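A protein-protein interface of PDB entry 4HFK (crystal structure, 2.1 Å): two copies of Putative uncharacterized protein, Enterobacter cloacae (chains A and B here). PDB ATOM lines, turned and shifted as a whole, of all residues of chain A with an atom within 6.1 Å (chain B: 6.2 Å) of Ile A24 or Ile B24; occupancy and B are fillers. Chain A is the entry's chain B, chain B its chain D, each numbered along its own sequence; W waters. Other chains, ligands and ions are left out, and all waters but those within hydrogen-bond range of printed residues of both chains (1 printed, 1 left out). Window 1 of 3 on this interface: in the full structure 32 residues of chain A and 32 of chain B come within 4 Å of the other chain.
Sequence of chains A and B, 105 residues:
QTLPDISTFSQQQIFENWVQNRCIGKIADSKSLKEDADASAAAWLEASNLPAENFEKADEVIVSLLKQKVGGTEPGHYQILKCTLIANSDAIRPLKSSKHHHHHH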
ATOM      1  N   VAL A  19      12.857   0.450 -17.310  1.00  0.00           N
ATOM      2  CA  VAL A  19      13.714   1.314 -16.494  1.00  0.00           C
ATOM      3  C   VAL A  19      15.187   1.081 -16.826  1.00  0.00           C
ATOM      4  O   VAL A  19      15.960   2.039 -16.981  1.00  0.00           O
ATOM      5  CB  VAL A  19      13.498   1.090 -14.977  1.00  0.00           C
ATOM      6  CG1 VAL A  19      14.563   1.843 -14.163  1.00  0.00           C
ATOM      7  CG2 VAL A  19      12.094   1.535 -14.559  1.00  0.00           C
ATOM      8  N   GLN A  20      15.574  -0.190 -16.937  1.00  0.00           N
ATOM      9  CA  GLN A  20      16.971  -0.532 -17.215  1.00  0.00           C
ATOM     10  C   GLN A  20      17.407  -0.020 -18.589  1.00  0.00           C
ATOM     11  O   GLN A  20      18.464   0.602 -18.725  1.00  0.00           O
ATOM     12  CB  GLN A  20      17.191  -2.048 -17.127  1.00  0.00           C
ATOM     13  CG  GLN A  20      18.654  -2.438 -16.851  1.00  0.00           C
ATOM     14  CD  GLN A  20      19.301  -3.201 -17.997  1.00  0.00           C
ATOM     15  OE1 GLN A  20      18.750  -3.278 -19.092  1.00  0.00           O
ATOM     16  NE2 GLN A  20      20.477  -3.777 -17.742  1.00  0.00           N
ATOM     17  N   ASN A  21      16.593  -0.285 -19.606  1.00  0.00           N
ATOM     18  CA  ASN A  21      16.932   0.116 -20.969  1.00  0.00           C
ATOM     19  C   ASN A  21      17.025   1.632 -21.075  1.00  0.00           C
ATOM     20  O   ASN A  21      17.918   2.175 -21.724  1.00  0.00           O
ATOM     21  CB  ASN A  21      15.898  -0.402 -21.966  1.00  0.00           C
ATOM     22  CG  ASN A  21      16.007  -1.892 -22.215  1.00  0.00           C
ATOM     23  OD1 ASN A  21      15.312  -2.424 -23.085  1.00  0.00           O
ATOM     24  ND2 ASN A  21      16.864  -2.582 -21.448  1.00  0.00           N
ATOM     25  N   ARG A  22      16.097   2.317 -20.425  1.00  0.00           N
ATOM     26  CA  ARG A  22      16.128   3.770 -20.391  1.00  0.00           C
ATOM     27  C   ARG A  22      17.365   4.308 -19.646  1.00  0.00           C
ATOM     28  O   ARG A  22      17.960   5.315 -20.053  1.00  0.00           O
ATOM     29  CB  ARG A  22      14.845   4.305 -19.767  1.00  0.00           C
ATOM     30  CG  ARG A  22      14.826   5.797 -19.662  1.00  0.00           C
ATOM     31  CD  ARG A  22      13.467   6.344 -20.044  1.00  0.00           C
ATOM     32  NE  ARG A  22      13.452   7.798 -19.939  1.00  0.00           N
ATOM     33  CZ  ARG A  22      13.515   8.618 -20.984  1.00  0.00           C
ATOM     34  NH1 ARG A  22      13.575   8.124 -22.216  1.00  0.00           N
ATOM     35  NH2 ARG A  22      13.498   9.927 -20.791  1.00  0.00           N
ATOM     36  N   CYS A  23      17.761   3.645 -18.561  1.00  0.00           N
ATOM     37  CA  CYS A  23      18.997   4.030 -17.878  1.00  0.00           C
ATOM     38  C   CYS A  23      20.202   3.899 -18.803  1.00  0.00           C
ATOM     39  O   CYS A  23      21.049   4.792 -18.859  1.00  0.00           O
ATOM     40  CB  CYS A  23      19.246   3.169 -16.643  1.00  0.00           C
ATOM     41  SG  CYS A  23      18.268   3.589 -15.231  1.00  0.00           S
ATOM     42  N   ILE A  24      20.283   2.775 -19.509  1.00  0.00           N
ATOM     43  CA  ILE A  24      21.368   2.548 -20.466  1.00  0.00           C
ATOM     44  C   ILE A  24      21.427   3.686 -21.477  1.00  0.00           C
ATOM     45  O   ILE A  24      22.508   4.169 -21.809  1.00  0.00           O
ATOM     46  CB  ILE A  24      21.204   1.198 -21.184  1.00  0.00           C
ATOM     47  CG1 ILE A  24      21.432   0.057 -20.184  1.00  0.00           C
ATOM     48  CG2 ILE A  24      22.193   1.076 -22.336  1.00  0.00           C
ATOM     49  CD1 ILE A  24      21.070  -1.318 -20.705  1.00  0.00           C
ATOM     50  N   GLY A  25      20.260   4.132 -21.936  1.00  0.00           N
ATOM     51  CA  GLY A  25      20.171   5.236 -22.873  1.00  0.00           C
ATOM     52  C   GLY A  25      20.712   6.531 -22.297  1.00  0.00           C
ATOM     53  O   GLY A  25      21.313   7.338 -23.011  1.00  0.00           O
ATOM     54  N   LYS A  26      20.497   6.741 -21.002  1.00  0.00           N
ATOM     55  CA  LYS A  26      20.978   7.945 -20.346  1.00  0.00           C
ATOM     56  C   LYS A  26      22.484   7.941 -20.089  1.00  0.00           C
ATOM     57  O   LYS A  26      23.092   9.003 -20.048  1.00  0.00           O
ATOM     58  CB  LYS A  26      20.234   8.172 -19.022  1.00  0.00           C
ATOM     59  CG  LYS A  26      18.779   8.571 -19.198  1.00  0.00           C
ATOM     60  CD  LYS A  26      18.143   8.899 -17.853  1.00  0.00           C
ATOM     61  CE  LYS A  26      16.655   9.185 -18.023  1.00  0.00           C
ATOM     62  NZ  LYS A  26      16.406  10.258 -19.035  1.00  0.00           N
ATOM     63  N   ILE A  27      23.085   6.766 -19.892  1.00  0.00           N
ATOM     64  CA  ILE A  27      24.523   6.710 -19.590  1.00  0.00           C
ATOM     65  C   ILE A  27      25.403   6.419 -20.809  1.00  0.00           C
ATOM     66  O   ILE A  27      26.620   6.569 -20.752  1.00  0.00           O
ATOM     67  CB  ILE A  27      24.873   5.692 -18.475  1.00  0.00           C
ATOM     68  CG1 ILE A  27      24.296   4.307 -18.782  1.00  0.00           C
ATOM     69  CG2 ILE A  27      24.367   6.168 -17.134  1.00  0.00           C
ATOM     70  CD1 ILE A  27      25.298   3.324 -19.314  1.00  0.00           C
ATOM     71  N   ALA A  28      24.788   5.981 -21.900  1.00  0.00           N
ATOM     72  CA  ALA A  28      25.542   5.611 -23.097  1.00  0.00           C
ATOM     73  C   ALA A  28      26.236   6.837 -23.699  1.00  0.00           C
ATOM     74  O   ALA A  28      25.598   7.863 -23.923  1.00  0.00           O
ATOM     75  CB  ALA A  28      24.635   4.977 -24.111  1.00  0.00           C
ATOM     76  N   ASP A  29      27.539   6.725 -23.938  1.00  0.00           N
ATOM     77  CA  ASP A  29      28.296   7.790 -24.596  1.00  0.00           C
ATOM     78  C   ASP A  29      28.337   7.403 -26.061  1.00  0.00           C
ATOM     79  O   ASP A  29      29.403   7.143 -26.626  1.00  0.00           O
ATOM     80  CB  ASP A  29      29.720   7.888 -24.030  1.00  0.00           C
ATOM     81  CG  ASP A  29      30.499   6.591 -24.185  1.00  0.00           C
ATOM     82  OD1 ASP A  29      29.880   5.507 -24.061  1.00  0.00           O
ATOM     83  OD2 ASP A  29      31.716   6.655 -24.480  1.00  0.00           O
ATOM     84  N   LEU A  33      23.779   3.970 -29.732  1.00  0.00           N
ATOM     85  CA  LEU A  33      23.398   3.070 -28.659  1.00  0.00           C
ATOM     86  C   LEU A  33      22.244   3.674 -27.865  1.00  0.00           C
ATOM     87  O   LEU A  33      21.329   2.960 -27.454  1.00  0.00           O
ATOM     88  CB  LEU A  33      24.587   2.739 -27.763  1.00  0.00           C
ATOM     89  CG  LEU A  33      24.441   1.481 -26.906  1.00  0.00           C
ATOM     90  CD1 LEU A  33      23.489   0.484 -27.542  1.00  0.00           C
ATOM     91  CD2 LEU A  33      25.783   0.840 -26.780  1.00  0.00           C
ATOM     92  N   LYS A  34      22.270   4.993 -27.685  1.00  0.00           N
ATOM     93  CA  LYS A  34      21.158   5.684 -27.044  1.00  0.00           C
ATOM     94  C   LYS A  34      19.850   5.516 -27.818  1.00  0.00           C
ATOM     95  O   LYS A  34      18.802   5.240 -27.219  1.00  0.00           O
ATOM     96  CB  LYS A  34      21.473   7.174 -26.848  1.00  0.00           C
ATOM     97  CG  LYS A  34      20.391   7.905 -26.070  1.00  0.00           C
ATOM     98  CD  LYS A  34      20.680   9.396 -25.951  1.00  0.00           C
ATOM     99  CE  LYS A  34      19.893  10.002 -24.790  1.00  0.00           C
ATOM    100  NZ  LYS A  34      18.528   9.418 -24.693  1.00  0.00           N
ATOM    101  N   ALA A  37      18.731   1.865 -27.306  1.00  0.00           N
ATOM    102  CA  ALA A  37      18.210   1.657 -25.963  1.00  0.00           C
ATOM    103  C   ALA A  37      16.829   2.301 -25.782  1.00  0.00           C
ATOM    104  O   ALA A  37      15.955   1.729 -25.123  1.00  0.00           O
ATOM    105  CB  ALA A  37      19.197   2.179 -24.925  1.00  0.00           C
ATOM    106  N   ILE A  80      26.566   0.115 -16.157  1.00  0.00           N
ATOM    107  CA  ILE A  80      25.691  -0.916 -16.716  1.00  0.00           C
ATOM    108  C   ILE A  80      25.076  -1.722 -15.573  1.00  0.00           C
ATOM    109  O   ILE A  80      23.862  -1.992 -15.560  1.00  0.00           O
ATOM    110  CB  ILE A  80      26.454  -1.848 -17.683  1.00  0.00           C
ATOM    111  CG1 ILE A  80      26.746  -1.119 -18.999  1.00  0.00           C
ATOM    112  CG2 ILE A  80      25.661  -3.132 -17.945  1.00  0.00           C
ATOM    113  CD1 ILE A  80      25.489  -0.745 -19.790  1.00  0.00           C
ATOM    114  N   CYS A  83      22.485   0.438 -13.794  1.00  0.00           N
ATOM    115  CA  CYS A  83      21.185   0.441 -14.467  1.00  0.00           C
ATOM    116  C   CYS A  83      20.273  -0.680 -13.927  1.00  0.00           C
ATOM    117  O   CYS A  83      19.067  -0.488 -13.754  1.00  0.00           O
ATOM    118  CB  CYS A  83      21.359   0.291 -15.984  1.00  0.00           C
ATOM    119  SG  CYS A  83      22.249   1.679 -16.790  1.00  0.00           S
ATOM    120  N   VAL B  19      24.579 -12.615 -18.449  1.00  0.00           N
ATOM    121  CA  VAL B  19      24.349 -12.800 -19.875  1.00  0.00           C
ATOM    122  C   VAL B  19      23.970 -11.497 -20.576  1.00  0.00           C
ATOM    123  O   VAL B  19      24.460 -11.216 -21.672  1.00  0.00           O
ATOM    124  CB  VAL B  19      23.255 -13.854 -20.147  1.00  0.00           C
ATOM    125  CG1 VAL B  19      22.929 -13.901 -21.642  1.00  0.00           C
ATOM    126  CG2 VAL B  19      23.722 -15.235 -19.665  1.00  0.00           C
ATOM    127  N   GLN B  20      23.107 -10.693 -19.954  1.00  0.00           N
ATOM    128  CA  GLN B  20      22.670  -9.459 -20.597  1.00  0.00           C
ATOM    129  C   GLN B  20      23.831  -8.485 -20.698  1.00  0.00           C
ATOM    130  O   GLN B  20      24.054  -7.877 -21.752  1.00  0.00           O
ATOM    131  CB  GLN B  20      21.501  -8.795 -19.850  1.00  0.00           C
ATOM    132  CG  GLN B  20      20.769  -7.785 -20.729  1.00  0.00           C
ATOM    133  CD  GLN B  20      20.649  -6.413 -20.106  1.00  0.00           C
ATOM    134  OE1 GLN B  20      21.455  -6.035 -19.255  1.00  0.00           O
ATOM    135  NE2 GLN B  20      19.633  -5.653 -20.528  1.00  0.00           N
ATOM    136  N   ASN B  21      24.564  -8.329 -19.601  1.00  0.00           N
ATOM    137  CA  ASN B  21      25.741  -7.463 -19.606  1.00  0.00           C
ATOM    138  C   ASN B  21      26.781  -7.885 -20.668  1.00  0.00           C
ATOM    139  O   ASN B  21      27.281  -7.041 -21.412  1.00  0.00           O
ATOM    140  CB  ASN B  21      26.397  -7.423 -18.221  1.00  0.00           C
ATOM    141  CG  ASN B  21      25.588  -6.643 -17.196  1.00  0.00           C
ATOM    142  OD1 ASN B  21      26.086  -6.366 -16.101  1.00  0.00           O
ATOM    143  ND2 ASN B  21      24.341  -6.297 -17.528  1.00  0.00           N
ATOM    144  N   ARG B  22      27.107  -9.179 -20.733  1.00  0.00           N
ATOM    145  CA  ARG B  22      28.051  -9.684 -21.741  1.00  0.00           C
ATOM    146  C   ARG B  22      27.543  -9.396 -23.150  1.00  0.00           C
ATOM    147  O   ARG B  22      28.316  -8.995 -24.036  1.00  0.00           O
ATOM    148  CB  ARG B  22      28.280 -11.199 -21.591  1.00  0.00           C
ATOM    149  CG  ARG B  22      29.007 -11.614 -20.305  1.00  0.00           C
ATOM    150  CD  ARG B  22      30.537 -11.515 -20.463  1.00  0.00           C
ATOM    151  NE  ARG B  22      31.026 -12.248 -21.641  1.00  0.00           N
ATOM    152  CZ  ARG B  22      32.241 -12.070 -22.160  1.00  0.00           C
ATOM    153  NH1 ARG B  22      33.056 -11.192 -21.598  1.00  0.00           N
ATOM    154  NH2 ARG B  22      32.640 -12.752 -23.226  1.00  0.00           N
ATOM    155  N   CYS B  23      26.247  -9.612 -23.361  1.00  0.00           N
ATOM    156  CA  CYS B  23      25.627  -9.291 -24.647  1.00  0.00           C
ATOM    157  C   CYS B  23      25.828  -7.818 -24.980  1.00  0.00           C
ATOM    158  O   CYS B  23      26.227  -7.471 -26.097  1.00  0.00           O
ATOM    159  CB  CYS B  23      24.130  -9.596 -24.627  1.00  0.00           C
ATOM    160  SG  CYS B  23      23.691 -11.336 -24.799  1.00  0.00           S
ATOM    161  N   ILE B  24      25.543  -6.947 -24.018  1.00  0.00           N
ATOM    162  CA  ILE B  24      25.747  -5.515 -24.239  1.00  0.00           C
ATOM    163  C   ILE B  24      27.198  -5.234 -24.623  1.00  0.00           C
ATOM    164  O   ILE B  24      27.464  -4.470 -25.553  1.00  0.00           O
ATOM    165  CB  ILE B  24      25.368  -4.685 -23.006  1.00  0.00           C
ATOM    166  CG1 ILE B  24      23.859  -4.780 -22.758  1.00  0.00           C
ATOM    167  CG2 ILE B  24      25.751  -3.224 -23.209  1.00  0.00           C
ATOM    168  CD1 ILE B  24      23.412  -4.117 -21.471  1.00  0.00           C
ATOM    169  N   GLY B  25      28.134  -5.882 -23.935  1.00  0.00           N
ATOM    170  CA  GLY B  25      29.549  -5.693 -24.210  1.00  0.00           C
ATOM    171  C   GLY B  25      29.938  -6.082 -25.629  1.00  0.00           C
ATOM    172  O   GLY B  25      30.906  -5.550 -26.180  1.00  0.00           O
ATOM    173  N   LYS B  26      29.190  -7.009 -26.225  1.00  0.00           N
ATOM    174  CA  LYS B  26      29.481  -7.454 -27.584  1.00  0.00           C
ATOM    175  C   LYS B  26      28.833  -6.588 -28.659  1.00  0.00           C
ATOM    176  O   LYS B  26      29.283  -6.604 -29.797  1.00  0.00           O
ATOM    177  CB  LYS B  26      29.058  -8.915 -27.788  1.00  0.00           C
ATOM    178  CG  LYS B  26      29.937  -9.939 -27.065  1.00  0.00           C
ATOM    179  CD  LYS B  26      29.361 -11.336 -27.261  1.00  0.00           C
ATOM    180  CE  LYS B  26      30.025 -12.358 -26.348  1.00  0.00           C
ATOM    181  NZ  LYS B  26      31.502 -12.342 -26.487  1.00  0.00           N
ATOM    182  N   ILE B  27      27.781  -5.843 -28.313  1.00  0.00           N
ATOM    183  CA  ILE B  27      27.090  -5.020 -29.319  1.00  0.00           C
ATOM    184  C   ILE B  27      27.383  -3.522 -29.227  1.00  0.00           C
ATOM    185  O   ILE B  27      27.069  -2.777 -30.150  1.00  0.00           O
ATOM    186  CB  ILE B  27      25.544  -5.254 -29.337  1.00  0.00           C
ATOM    187  CG1 ILE B  27      24.899  -4.918 -27.986  1.00  0.00           C
ATOM    188  CG2 ILE B  27      25.237  -6.692 -29.731  1.00  0.00           C
ATOM    189  CD1 ILE B  27      24.408  -3.480 -27.836  1.00  0.00           C
ATOM    190  N   ALA B  28      27.954  -3.085 -28.109  1.00  0.00           N
ATOM    191  CA  ALA B  28      28.226  -1.663 -27.891  1.00  0.00           C
ATOM    192  C   ALA B  28      29.297  -1.159 -28.853  1.00  0.00           C
ATOM    193  O   ALA B  28      30.310  -1.824 -29.064  1.00  0.00           O
ATOM    194  CB  ALA B  28      28.668  -1.426 -26.459  1.00  0.00           C
ATOM    195  N   ASP B  29      29.085   0.017 -29.429  1.00  0.00           N
ATOM    196  CA  ASP B  29      30.122   0.614 -30.263  1.00  0.00           C
ATOM    197  C   ASP B  29      31.169   1.336 -29.409  1.00  0.00           C
ATOM    198  O   ASP B  29      32.361   1.347 -29.724  1.00  0.00           O
ATOM    199  CB  ASP B  29      29.512   1.540 -31.328  1.00  0.00           C
ATOM    200  CG  ASP B  29      28.518   2.537 -30.753  1.00  0.00           C
ATOM    201  OD1 ASP B  29      28.176   2.430 -29.551  1.00  0.00           O
ATOM    202  OD2 ASP B  29      28.058   3.415 -31.523  1.00  0.00           O
ATOM    203  N   LEU B  33      31.783   2.036 -23.030  1.00  0.00           N
ATOM    204  CA  LEU B  33      30.606   1.260 -22.647  1.00  0.00           C
ATOM    205  C   LEU B  33      30.869  -0.248 -22.665  1.00  0.00           C
ATOM    206  O   LEU B  33      30.377  -0.977 -21.794  1.00  0.00           O
ATOM    207  CB  LEU B  33      29.371   1.608 -23.482  1.00  0.00           C
ATOM    208  CG  LEU B  33      28.157   1.032 -22.744  1.00  0.00           C
ATOM    209  CD1 LEU B  33      27.521   2.083 -21.850  1.00  0.00           C
ATOM    210  CD2 LEU B  33      27.145   0.408 -23.667  1.00  0.00           C
ATOM    211  N   LYS B  34      31.645  -0.718 -23.642  1.00  0.00           N
ATOM    212  CA  LYS B  34      32.060  -2.123 -23.662  1.00  0.00           C
ATOM    213  C   LYS B  34      32.812  -2.512 -22.389  1.00  0.00           C
ATOM    214  O   LYS B  34      32.541  -3.560 -21.801  1.00  0.00           O
ATOM    215  CB  LYS B  34      32.925  -2.441 -24.894  1.00  0.00           C
ATOM    216  CG  LYS B  34      32.128  -2.521 -26.193  1.00  0.00           C
ATOM    217  CD  LYS B  34      32.941  -3.110 -27.352  1.00  0.00           C
ATOM    218  CE  LYS B  34      33.951  -2.118 -27.916  1.00  0.00           C
ATOM    219  NZ  LYS B  34      34.174  -2.352 -29.379  1.00  0.00           N
ATOM    220  N   ALA B  37      30.451  -2.591 -19.464  1.00  0.00           N
ATOM    221  CA  ALA B  37      29.578  -3.756 -19.579  1.00  0.00           C
ATOM    222  C   ALA B  37      30.289  -5.037 -19.149  1.00  0.00           C
ATOM    223  O   ALA B  37      29.717  -5.859 -18.429  1.00  0.00           O
ATOM    224  CB  ALA B  37      29.037  -3.893 -20.995  1.00  0.00           C
ATOM    225  N   ASP B  38      31.533  -5.209 -19.583  1.00  0.00           N
ATOM    226  CA  ASP B  38      32.278  -6.408 -19.221  1.00  0.00           C
ATOM    227  C   ASP B  38      32.756  -6.365 -17.773  1.00  0.00           C
ATOM    228  O   ASP B  38      32.901  -7.407 -17.136  1.00  0.00           O
ATOM    229  CB  ASP B  38      33.463  -6.644 -20.169  1.00  0.00           C
ATOM    230  CG  ASP B  38      33.019  -7.031 -21.567  1.00  0.00           C
ATOM    231  OD1 ASP B  38      31.852  -7.435 -21.725  1.00  0.00           O
ATOM    232  OD2 ASP B  38      33.835  -6.937 -22.510  1.00  0.00           O
ATOM    233  N   ILE B  80      19.631  -3.662 -27.699  1.00  0.00           N
ATOM    234  CA  ILE B  80      19.523  -3.625 -26.242  1.00  0.00           C
ATOM    235  C   ILE B  80      18.348  -4.514 -25.800  1.00  0.00           C
ATOM    236  O   ILE B  80      18.459  -5.273 -24.832  1.00  0.00           O
ATOM    237  CB  ILE B  80      19.370  -2.182 -25.723  1.00  0.00           C
ATOM    238  CG1 ILE B  80      20.695  -1.428 -25.858  1.00  0.00           C
ATOM    239  CG2 ILE B  80      18.876  -2.161 -24.275  1.00  0.00           C
ATOM    240  CD1 ILE B  80      21.817  -1.982 -25.009  1.00  0.00           C
ATOM    241  N   CYS B  83      19.490  -8.167 -26.188  1.00  0.00           N
ATOM    242  CA  CYS B  83      20.332  -8.621 -25.075  1.00  0.00           C
ATOM    243  C   CYS B  83      19.496  -9.231 -23.935  1.00  0.00           C
ATOM    244  O   CYS B  83      19.867 -10.265 -23.353  1.00  0.00           O
ATOM    245  CB  CYS B  83      21.206  -7.465 -24.553  1.00  0.00           C
ATOM    246  SG  CYS B  83      22.477  -6.867 -25.742  1.00  0.00           S
HETATM  247  O   HOH W   1      23.269  -4.774 -15.192  1.00  0.00           O
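OE1 of Gln A20 lies within hydrogen-bond range of ND2 of Asn A21.
The side-chain amide oxygen of Gln B20 sits at hydrogen-bond distance from the side-chain amide nitrogen of Asn B21, at 3.4 Å.
The backbone NH (N) of Ile A24 is in hydrogen-bond range of the side-chain sulfur (SG) of Cys A83, at 3.5 Å.
N of Ile B24 is in hydrogen-bond range of SG of Cys B83 (3.5 Å).
The side-chain amide nitrogen of Gln A20 lies within hydrogen-bond range of the side-chain amide oxygen of Gln B20, 2.9 Å away.
Gln B20 touches its own counterpart, Gln A20.
Ile A27 touches Leu B33, but with the chains exchanged Leu A33 does not touch Ile B27 (4.1 Å).
Leu A33 touches its own counterpart, Leu B33.
Leu A33 touches Ile B80, but with the chains exchanged Ile A80 does not touch Leu B33 (4.05 Å).
16 positions are printed for both chains.
Among the printed residues, merely in contact across the chains: Leu A33 with Leu B33 (3.4 Å), Ile A80 with Asn B21 (3.5 Å), Asn A21 with Ile B80 (3.5 Å), Ile A27 with Leu B33 (3.6 Å), Leu A33 with Ala B28 (3.7 Å), Ile A24 with Ile B24 (3.7 Å), Leu A33 with Ile B80 (3.8 Å), Ile A80 with Ala B37 (3.9 Å), Ala A37 with Ile B80 (3.96 Å), Asp A29 with Leu B33 (3.97 Å) and Leu A33 with Asp B29 (3.99 Å).
Water W1 lies within hydrogen-bond range of the backbone carbonyl oxygen (O) of Ile A80 (2.9 Å) and the side-chain amide nitrogen (ND2) of Asn B21 (3.0 Å).
Of chain B, only Ile B24 (3.7 Å) comes within 4 Å of Ile A24.
Of the printed residues of chain B, Ala A37 touches Ile B80 (3.96 Å).
Of the printed residues of chain A, Asn B21 touches Ile A80 (3.5 Å).
Of chain A, only Ile A24 (3.7 Å) comes within 4 Å of Ile B24.
Of the printed residues of chain A, Ile B80 touches Asn A21, Leu A33 and Ala A37.
The nearest printed residue of chain B that does not touch Asn A21 is Gln B20 (4.2 Å).
Along chain A the printed residues that touch a printed residue of chain B span positions 20 to 80.
Of the 17 printed residues of chain B, 8 touch a printed residue of chain A.
Printed residues of chain B that touch a printed residue of chain A: Gln B20, Asn B21, Ile B24, Ala B28, Asp B29, Leu B33, Ala B37 and Ile B80.
Hydrophobic or aromatic side chains of chain B that line the printed part of chain A: Ile B24, Ala B28, Leu B33 and Ile B80.
Among the printed residues, 12 pairs touch across the chains.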
